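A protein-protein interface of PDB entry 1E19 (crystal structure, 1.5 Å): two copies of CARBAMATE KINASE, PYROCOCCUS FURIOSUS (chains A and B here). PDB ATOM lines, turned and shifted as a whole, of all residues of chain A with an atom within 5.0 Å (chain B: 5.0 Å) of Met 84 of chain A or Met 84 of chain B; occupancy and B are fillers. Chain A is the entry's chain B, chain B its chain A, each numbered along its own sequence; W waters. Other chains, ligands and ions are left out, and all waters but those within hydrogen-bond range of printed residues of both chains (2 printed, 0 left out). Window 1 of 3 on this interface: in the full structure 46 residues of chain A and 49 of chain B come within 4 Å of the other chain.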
ATOM      1  N   LEU A  60     -26.795 -20.928 -19.205  1.00  0.00           N
ATOM      2  CA  LEU A  60     -27.019 -19.668 -19.917  1.00  0.00           C
ATOM      3  C   LEU A  60     -26.317 -19.573 -21.299  1.00  0.00           C
ATOM      4  O   LEU A  60     -26.985 -19.003 -22.146  1.00  0.00           O
ATOM      5  CB  LEU A  60     -26.597 -18.508 -18.969  1.00  0.00           C
ATOM      6  CG  LEU A  60     -27.568 -18.248 -17.773  1.00  0.00           C
ATOM      7  CD1 LEU A  60     -26.818 -17.412 -16.725  1.00  0.00           C
ATOM      8  CD2 LEU A  60     -28.780 -17.484 -18.293  1.00  0.00           C
ATOM      9  N   MET A  64     -28.429 -19.023 -24.761  1.00  0.00           N
ATOM     10  CA  MET A  64     -28.243 -17.897 -25.633  1.00  0.00           C
ATOM     11  C   MET A  64     -27.742 -18.373 -27.045  1.00  0.00           C
ATOM     12  O   MET A  64     -28.108 -17.657 -27.917  1.00  0.00           O
ATOM     13  CB  MET A  64     -27.240 -16.863 -24.987  1.00  0.00           C
ATOM     14  CG  MET A  64     -27.950 -16.224 -23.760  1.00  0.00           C
ATOM     15  SD  MET A  64     -26.922 -14.828 -23.088  1.00  0.00           S
ATOM     16  CE  MET A  64     -25.596 -15.633 -22.338  1.00  0.00           C
ATOM     17  N   GLN A  76     -25.095 -13.001 -25.359  1.00  0.00           N
ATOM     18  CA  GLN A  76     -24.183 -12.102 -24.594  1.00  0.00           C
ATOM     19  C   GLN A  76     -22.946 -12.824 -24.199  1.00  0.00           C
ATOM     20  O   GLN A  76     -22.899 -14.037 -24.007  1.00  0.00           O
ATOM     21  CB  GLN A  76     -24.906 -11.759 -23.250  1.00  0.00           C
ATOM     22  CG  GLN A  76     -26.232 -10.997 -23.497  1.00  0.00           C
ATOM     23  CD  GLN A  76     -26.061  -9.641 -24.238  1.00  0.00           C
ATOM     24  OE1 GLN A  76     -25.028  -9.006 -24.036  1.00  0.00           O
ATOM     25  NE2 GLN A  76     -27.014  -9.147 -25.007  1.00  0.00           N
ATOM     26  N   VAL A  80     -21.049 -11.055 -19.017  1.00  0.00           N
ATOM     27  CA  VAL A  80     -22.460 -10.855 -18.793  1.00  0.00           C
ATOM     28  C   VAL A  80     -23.113 -12.127 -18.277  1.00  0.00           C
ATOM     29  O   VAL A  80     -23.906 -12.078 -17.293  1.00  0.00           O
ATOM     30  CB  VAL A  80     -23.159 -10.348 -20.079  1.00  0.00           C
ATOM     31  CG1 VAL A  80     -24.663 -10.441 -19.860  1.00  0.00           C
ATOM     32  CG2 VAL A  80     -22.617  -8.930 -20.317  1.00  0.00           C
ATOM     33  N   ALA A  81     -22.799 -13.330 -18.787  1.00  0.00           N
ATOM     34  CA  ALA A  81     -23.390 -14.569 -18.263  1.00  0.00           C
ATOM     35  C   ALA A  81     -23.021 -14.758 -16.820  1.00  0.00           C
ATOM     36  O   ALA A  81     -23.906 -15.180 -16.033  1.00  0.00           O
ATOM     37  CB  ALA A  81     -22.905 -15.735 -19.154  1.00  0.00           C
ATOM     38  N   GLY A  82     -21.811 -14.352 -16.424  1.00  0.00           N
ATOM     39  CA  GLY A  82     -21.453 -14.522 -14.991  1.00  0.00           C
ATOM     40  C   GLY A  82     -22.256 -13.551 -14.158  1.00  0.00           C
ATOM     41  O   GLY A  82     -22.764 -13.983 -13.109  1.00  0.00           O
ATOM     42  N   ALA A  83     -22.462 -12.309 -14.622  1.00  0.00           N
ATOM     43  CA  ALA A  83     -23.305 -11.367 -13.827  1.00  0.00           C
ATOM     44  C   ALA A  83     -24.724 -11.866 -13.732  1.00  0.00           C
ATOM     45  O   ALA A  83     -25.372 -11.780 -12.655  1.00  0.00           O
ATOM     46  CB  ALA A  83     -23.243 -10.003 -14.551  1.00  0.00           C
ATOM     47  N   MET A  84     -25.282 -12.418 -14.812  1.00  0.00           N
ATOM     48  CA  MET A  84     -26.645 -13.020 -14.748  1.00  0.00           C
ATOM     49  C   MET A  84     -26.686 -14.142 -13.715  1.00  0.00           C
ATOM     50  O   MET A  84     -27.623 -14.217 -12.932  1.00  0.00           O
ATOM     51  CB  MET A  84     -27.004 -13.642 -16.126  1.00  0.00           C
ATOM     52  CG  MET A  84     -27.221 -12.597 -17.229  1.00  0.00           C
ATOM     53  SD  MET A  84     -27.320 -13.557 -18.826  1.00  0.00           S
ATOM     54  CE  MET A  84     -27.868 -12.337 -19.967  1.00  0.00           C
ATOM     55  N   SER A  85     -25.639 -14.981 -13.699  1.00  0.00           N
ATOM     56  CA  SER A  85     -25.628 -16.095 -12.721  1.00  0.00           C
ATOM     57  C   SER A  85     -25.595 -15.593 -11.291  1.00  0.00           C
ATOM     58  O   SER A  85     -26.091 -16.258 -10.393  1.00  0.00           O
ATOM     59  CB  SER A  85     -24.491 -17.106 -13.034  1.00  0.00           C
ATOM     60  OG  SER A  85     -23.200 -16.596 -12.619  1.00  0.00           O
ATOM     61  N   GLN A  86     -24.826 -14.520 -11.066  1.00  0.00           N
ATOM     62  CA  GLN A  86     -24.769 -13.994  -9.662  1.00  0.00           C
ATOM     63  C   GLN A  86     -26.146 -13.509  -9.253  1.00  0.00           C
ATOM     64  O   GLN A  86     -26.494 -13.730  -8.056  1.00  0.00           O
ATOM     65  CB  GLN A  86     -23.799 -12.819  -9.586  1.00  0.00           C
ATOM     66  CG  GLN A  86     -22.314 -13.195  -9.721  1.00  0.00           C
ATOM     67  CD  GLN A  86     -21.437 -11.957  -9.461  1.00  0.00           C
ATOM     68  OE1 GLN A  86     -21.659 -11.153  -8.551  1.00  0.00           O
ATOM     69  NE2 GLN A  86     -20.370 -11.931 -10.286  1.00  0.00           N
ATOM     70  N   GLY A  87     -26.900 -12.835 -10.137  1.00  0.00           N
ATOM     71  CA  GLY A  87     -28.243 -12.365  -9.725  1.00  0.00           C
ATOM     72  C   GLY A  87     -29.176 -13.585  -9.470  1.00  0.00           C
ATOM     73  O   GLY A  87     -29.863 -13.626  -8.465  1.00  0.00           O
ATOM     74  N   TRP A  88     -29.103 -14.553 -10.369  1.00  0.00           N
ATOM     75  CA  TRP A  88     -29.953 -15.805 -10.232  1.00  0.00           C
ATOM     76  C   TRP A  88     -29.668 -16.534  -8.915  1.00  0.00           C
ATOM     77  O   TRP A  88     -30.617 -16.735  -8.106  1.00  0.00           O
ATOM     78  CB  TRP A  88     -29.561 -16.654 -11.437  1.00  0.00           C
ATOM     79  CG  TRP A  88     -30.178 -18.033 -11.507  1.00  0.00           C
ATOM     80  CD1 TRP A  88     -31.117 -18.641 -10.669  1.00  0.00           C
ATOM     81  CD2 TRP A  88     -29.839 -18.996 -12.476  1.00  0.00           C
ATOM     82  NE1 TRP A  88     -31.390 -19.907 -11.176  1.00  0.00           N
ATOM     83  CE2 TRP A  88     -30.613 -20.156 -12.293  1.00  0.00           C
ATOM     84  CE3 TRP A  88     -28.932 -19.007 -13.573  1.00  0.00           C
ATOM     85  CZ2 TRP A  88     -30.505 -21.324 -13.071  1.00  0.00           C
ATOM     86  CZ3 TRP A  88     -28.813 -20.140 -14.355  1.00  0.00           C
ATOM     87  CH2 TRP A  88     -29.602 -21.221 -14.130  1.00  0.00           C
ATOM     88  N   LEU B  60     -34.203 -12.720 -22.255  1.00  0.00           N
ATOM     89  CA  LEU B  60     -33.982 -13.949 -21.517  1.00  0.00           C
ATOM     90  C   LEU B  60     -35.157 -14.965 -21.670  1.00  0.00           C
ATOM     91  O   LEU B  60     -34.804 -16.138 -21.680  1.00  0.00           O
ATOM     92  CB  LEU B  60     -33.754 -13.559 -20.054  1.00  0.00           C
ATOM     93  CG  LEU B  60     -32.383 -12.955 -19.782  1.00  0.00           C
ATOM     94  CD1 LEU B  60     -32.391 -12.289 -18.397  1.00  0.00           C
ATOM     95  CD2 LEU B  60     -31.348 -14.045 -19.749  1.00  0.00           C
ATOM     96  N   MET B  64     -34.432 -18.694 -23.115  1.00  0.00           N
ATOM     97  CA  MET B  64     -34.695 -19.944 -22.402  1.00  0.00           C
ATOM     98  C   MET B  64     -35.808 -20.775 -23.093  1.00  0.00           C
ATOM     99  O   MET B  64     -35.663 -21.996 -22.947  1.00  0.00           O
ATOM    100  CB  MET B  64     -35.097 -19.641 -20.924  1.00  0.00           C
ATOM    101  CG  MET B  64     -33.867 -19.041 -20.163  1.00  0.00           C
ATOM    102  SD  MET B  64     -34.228 -18.837 -18.387  1.00  0.00           S
ATOM    103  CE  MET B  64     -35.367 -17.464 -18.343  1.00  0.00           C
ATOM    104  N   GLN B  76     -36.196 -21.164 -16.791  1.00  0.00           N
ATOM    105  CA  GLN B  76     -36.462 -20.704 -15.379  1.00  0.00           C
ATOM    106  C   GLN B  76     -37.613 -19.718 -15.481  1.00  0.00           C
ATOM    107  O   GLN B  76     -37.902 -19.029 -16.443  1.00  0.00           O
ATOM    108  CB  GLN B  76     -35.228 -19.951 -14.926  1.00  0.00           C
ATOM    109  CG  GLN B  76     -33.939 -20.851 -14.915  1.00  0.00           C
ATOM    110  CD  GLN B  76     -34.104 -21.993 -13.908  1.00  0.00           C
ATOM    111  OE1 GLN B  76     -34.699 -21.821 -12.888  1.00  0.00           O
ATOM    112  NE2 GLN B  76     -33.431 -23.093 -14.154  1.00  0.00           N
ATOM    113  N   VAL B  80     -36.880 -15.595 -11.376  1.00  0.00           N
ATOM    114  CA  VAL B  80     -35.465 -15.828 -11.650  1.00  0.00           C
ATOM    115  C   VAL B  80     -34.988 -15.023 -12.831  1.00  0.00           C
ATOM    116  O   VAL B  80     -33.859 -14.474 -12.757  1.00  0.00           O
ATOM    117  CB  VAL B  80     -35.268 -17.367 -11.838  1.00  0.00           C
ATOM    118  CG1 VAL B  80     -33.903 -17.613 -12.388  1.00  0.00           C
ATOM    119  CG2 VAL B  80     -35.478 -18.112 -10.502  1.00  0.00           C
ATOM    120  N   ALA B  81     -35.741 -14.896 -13.921  1.00  0.00           N
ATOM    121  CA  ALA B  81     -35.251 -14.059 -15.050  1.00  0.00           C
ATOM    122  C   ALA B  81     -35.126 -12.623 -14.604  1.00  0.00           C
ATOM    123  O   ALA B  81     -34.166 -11.956 -15.114  1.00  0.00           O
ATOM    124  CB  ALA B  81     -36.318 -14.124 -16.184  1.00  0.00           C
ATOM    125  N   GLY B  82     -35.988 -12.101 -13.715  1.00  0.00           N
ATOM    126  CA  GLY B  82     -35.776 -10.735 -13.259  1.00  0.00           C
ATOM    127  C   GLY B  82     -34.506 -10.607 -12.462  1.00  0.00           C
ATOM    128  O   GLY B  82     -33.710  -9.630 -12.668  1.00  0.00           O
ATOM    129  N   ALA B  83     -34.172 -11.602 -11.586  1.00  0.00           N
ATOM    130  CA  ALA B  83     -32.881 -11.570 -10.891  1.00  0.00           C
ATOM    131  C   ALA B  83     -31.689 -11.585 -11.838  1.00  0.00           C
ATOM    132  O   ALA B  83     -30.679 -10.919 -11.643  1.00  0.00           O
ATOM    133  CB  ALA B  83     -32.795 -12.814  -9.958  1.00  0.00           C
ATOM    134  N   MET B  84     -31.736 -12.457 -12.875  1.00  0.00           N
ATOM    135  CA  MET B  84     -30.681 -12.498 -13.889  1.00  0.00           C
ATOM    136  C   MET B  84     -30.540 -11.109 -14.542  1.00  0.00           C
ATOM    137  O   MET B  84     -29.344 -10.673 -14.664  1.00  0.00           O
ATOM    138  CB  MET B  84     -31.088 -13.482 -15.035  1.00  0.00           C
ATOM    139  CG  MET B  84     -30.985 -14.980 -14.548  1.00  0.00           C
ATOM    140  SD  MET B  84     -31.813 -15.893 -15.958  1.00  0.00           S
ATOM    141  CE  MET B  84     -31.600 -17.612 -15.477  1.00  0.00           C
ATOM    142  N   SER B  85     -31.645 -10.425 -14.798  1.00  0.00           N
ATOM    143  CA  SER B  85     -31.553  -9.118 -15.451  1.00  0.00           C
ATOM    144  C   SER B  85     -30.930  -8.051 -14.534  1.00  0.00           C
ATOM    145  O   SER B  85     -30.280  -7.140 -15.039  1.00  0.00           O
ATOM    146  CB  SER B  85     -32.934  -8.606 -15.964  1.00  0.00           C
ATOM    147  OG  SER B  85     -33.791  -8.117 -14.907  1.00  0.00           O
ATOM    148  N   GLN B  86     -31.252  -8.179 -13.231  1.00  0.00           N
ATOM    149  CA  GLN B  86     -30.615  -7.184 -12.290  1.00  0.00           C
ATOM    150  C   GLN B  86     -29.108  -7.408 -12.250  1.00  0.00           C
ATOM    151  O   GLN B  86     -28.366  -6.403 -12.184  1.00  0.00           O
ATOM    152  CB  GLN B  86     -31.158  -7.425 -10.835  1.00  0.00           C
ATOM    153  CG  GLN B  86     -32.638  -6.986 -10.710  1.00  0.00           C
ATOM    154  CD  GLN B  86     -32.995  -7.010  -9.233  1.00  0.00           C
ATOM    155  OE1 GLN B  86     -32.262  -6.691  -8.328  1.00  0.00           O
ATOM    156  NE2 GLN B  86     -34.241  -7.523  -8.963  1.00  0.00           N
ATOM    157  N   GLY B  87     -28.647  -8.666 -12.274  1.00  0.00           N
ATOM    158  CA  GLY B  87     -27.214  -8.864 -12.282  1.00  0.00           C
ATOM    159  C   GLY B  87     -26.546  -8.318 -13.589  1.00  0.00           C
ATOM    160  O   GLY B  87     -25.493  -7.666 -13.519  1.00  0.00           O
ATOM    161  N   TRP B  88     -27.189  -8.627 -14.702  1.00  0.00           N
ATOM    162  CA  TRP B  88     -26.651  -8.175 -16.015  1.00  0.00           C
ATOM    163  C   TRP B  88     -26.619  -6.656 -16.156  1.00  0.00           C
ATOM    164  O   TRP B  88     -25.488  -6.128 -16.376  1.00  0.00           O
ATOM    165  CB  TRP B  88     -27.683  -8.702 -16.994  1.00  0.00           C
ATOM    166  CG  TRP B  88     -27.494  -8.307 -18.465  1.00  0.00           C
ATOM    167  CD1 TRP B  88     -26.424  -7.625 -18.994  1.00  0.00           C
ATOM    168  CD2 TRP B  88     -28.442  -8.625 -19.497  1.00  0.00           C
ATOM    169  NE1 TRP B  88     -26.698  -7.500 -20.369  1.00  0.00           N
ATOM    170  CE2 TRP B  88     -27.892  -8.134 -20.720  1.00  0.00           C
ATOM    171  CE3 TRP B  88     -29.680  -9.295 -19.523  1.00  0.00           C
ATOM    172  CZ2 TRP B  88     -28.606  -8.226 -21.917  1.00  0.00           C
ATOM    173  CZ3 TRP B  88     -30.362  -9.418 -20.743  1.00  0.00           C
ATOM    174  CH2 TRP B  88     -29.812  -8.941 -21.923  1.00  0.00           C
HETATM  175  O   HOH W   1     -33.384 -22.058 -10.644  1.00  0.00           O
HETATM  176  O   HOH W   2     -25.206  -6.607 -22.802  1.00  0.00           O
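N of Gln 76 of chain A lies within hydrogen-bond range of SD of Met 64 of chain A.
N of Gln 76 of chain B lies within hydrogen-bond range of SD of Met 64 of chain B.
Water W1 bridges OE1 of Gln 76 of chain B and NE1 of Trp 88 of chain A.
Water W2 lies within hydrogen-bond range of the side-chain amide oxygen of Gln 76 of chain A (2.7 Å) and the indole nitrogen of Trp 88 of chain B (3.0 Å).
Of chain B, only Leu 60 (3.9 Å), Met 84 (3.6 Å) and Trp 88 (3.6 Å) come within 4 Å of Met 84 of chain A.
Of the printed residues of chain B, Gly 87 of chain A touches Ala 83 (3.4 Å).
Printed residues of chain A within 4 Å of Val 80 of chain B: Trp 88.
Of the printed residues of chain A, Met 84 of chain B touches Leu 60, Met 84 and Trp 88.
The nearest residue of chain B that does not touch Met 84 of chain A is Gly 87 of chain B (4.5 Å).
Leu 60 of chain A touches Met 84 of chain B, and with the chains exchanged Met 84 of chain A touches Leu 60 of chain B.
Gln 76 of chain A touches Trp 88 of chain B, and with the chains exchanged Trp 88 of chain A touches Gln 76 of chain B.
Ala 83 of chain A touches Gly 87 of chain B, and with the chains exchanged Gly 87 of chain A touches Ala 83 of chain B.
Met 84 of chain A touches Trp 88 of chain B, and with the chains exchanged Trp 88 of chain A touches Met 84 of chain B.
Hydrophobic or aromatic side chains of chain B that line the printed part of chain A: Leu 60, Val 80, Ala 83, Met 84 and Trp 88.
Among the printed residues, no Asp or Glu carboxylate lies within 4 Å of a Lys or Arg side-chain nitrogen of the other chain.
Among the printed residues, pairs that only touch across the chains: Gly 87 of chain A with Ala 83 of chain B (3.4 Å), Ala 83 of chain A with Gly 87 of chain B (3.4 Å), Trp 88 of chain A with Val 80 of chain B (3.4 Å), Val 80 of chain A with Trp 88 of chain B (3.4 Å), Trp 88 of chain A with Met 84 of chain B (3.6 Å), Met 84 of chain A with Trp 88 of chain B (3.6 Å), Met 84 of chain A with Met 84 of chain B (3.6 Å), Trp 88 of chain A with Gln 76 of chain B (3.6 Å), Gln 76 of chain A with Trp 88 of chain B (3.6 Å), Met 84 of chain A with Leu 60 of chain B (3.9 Å) and Leu 60 of chain A with Met 84 of chain B (3.99 Å).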
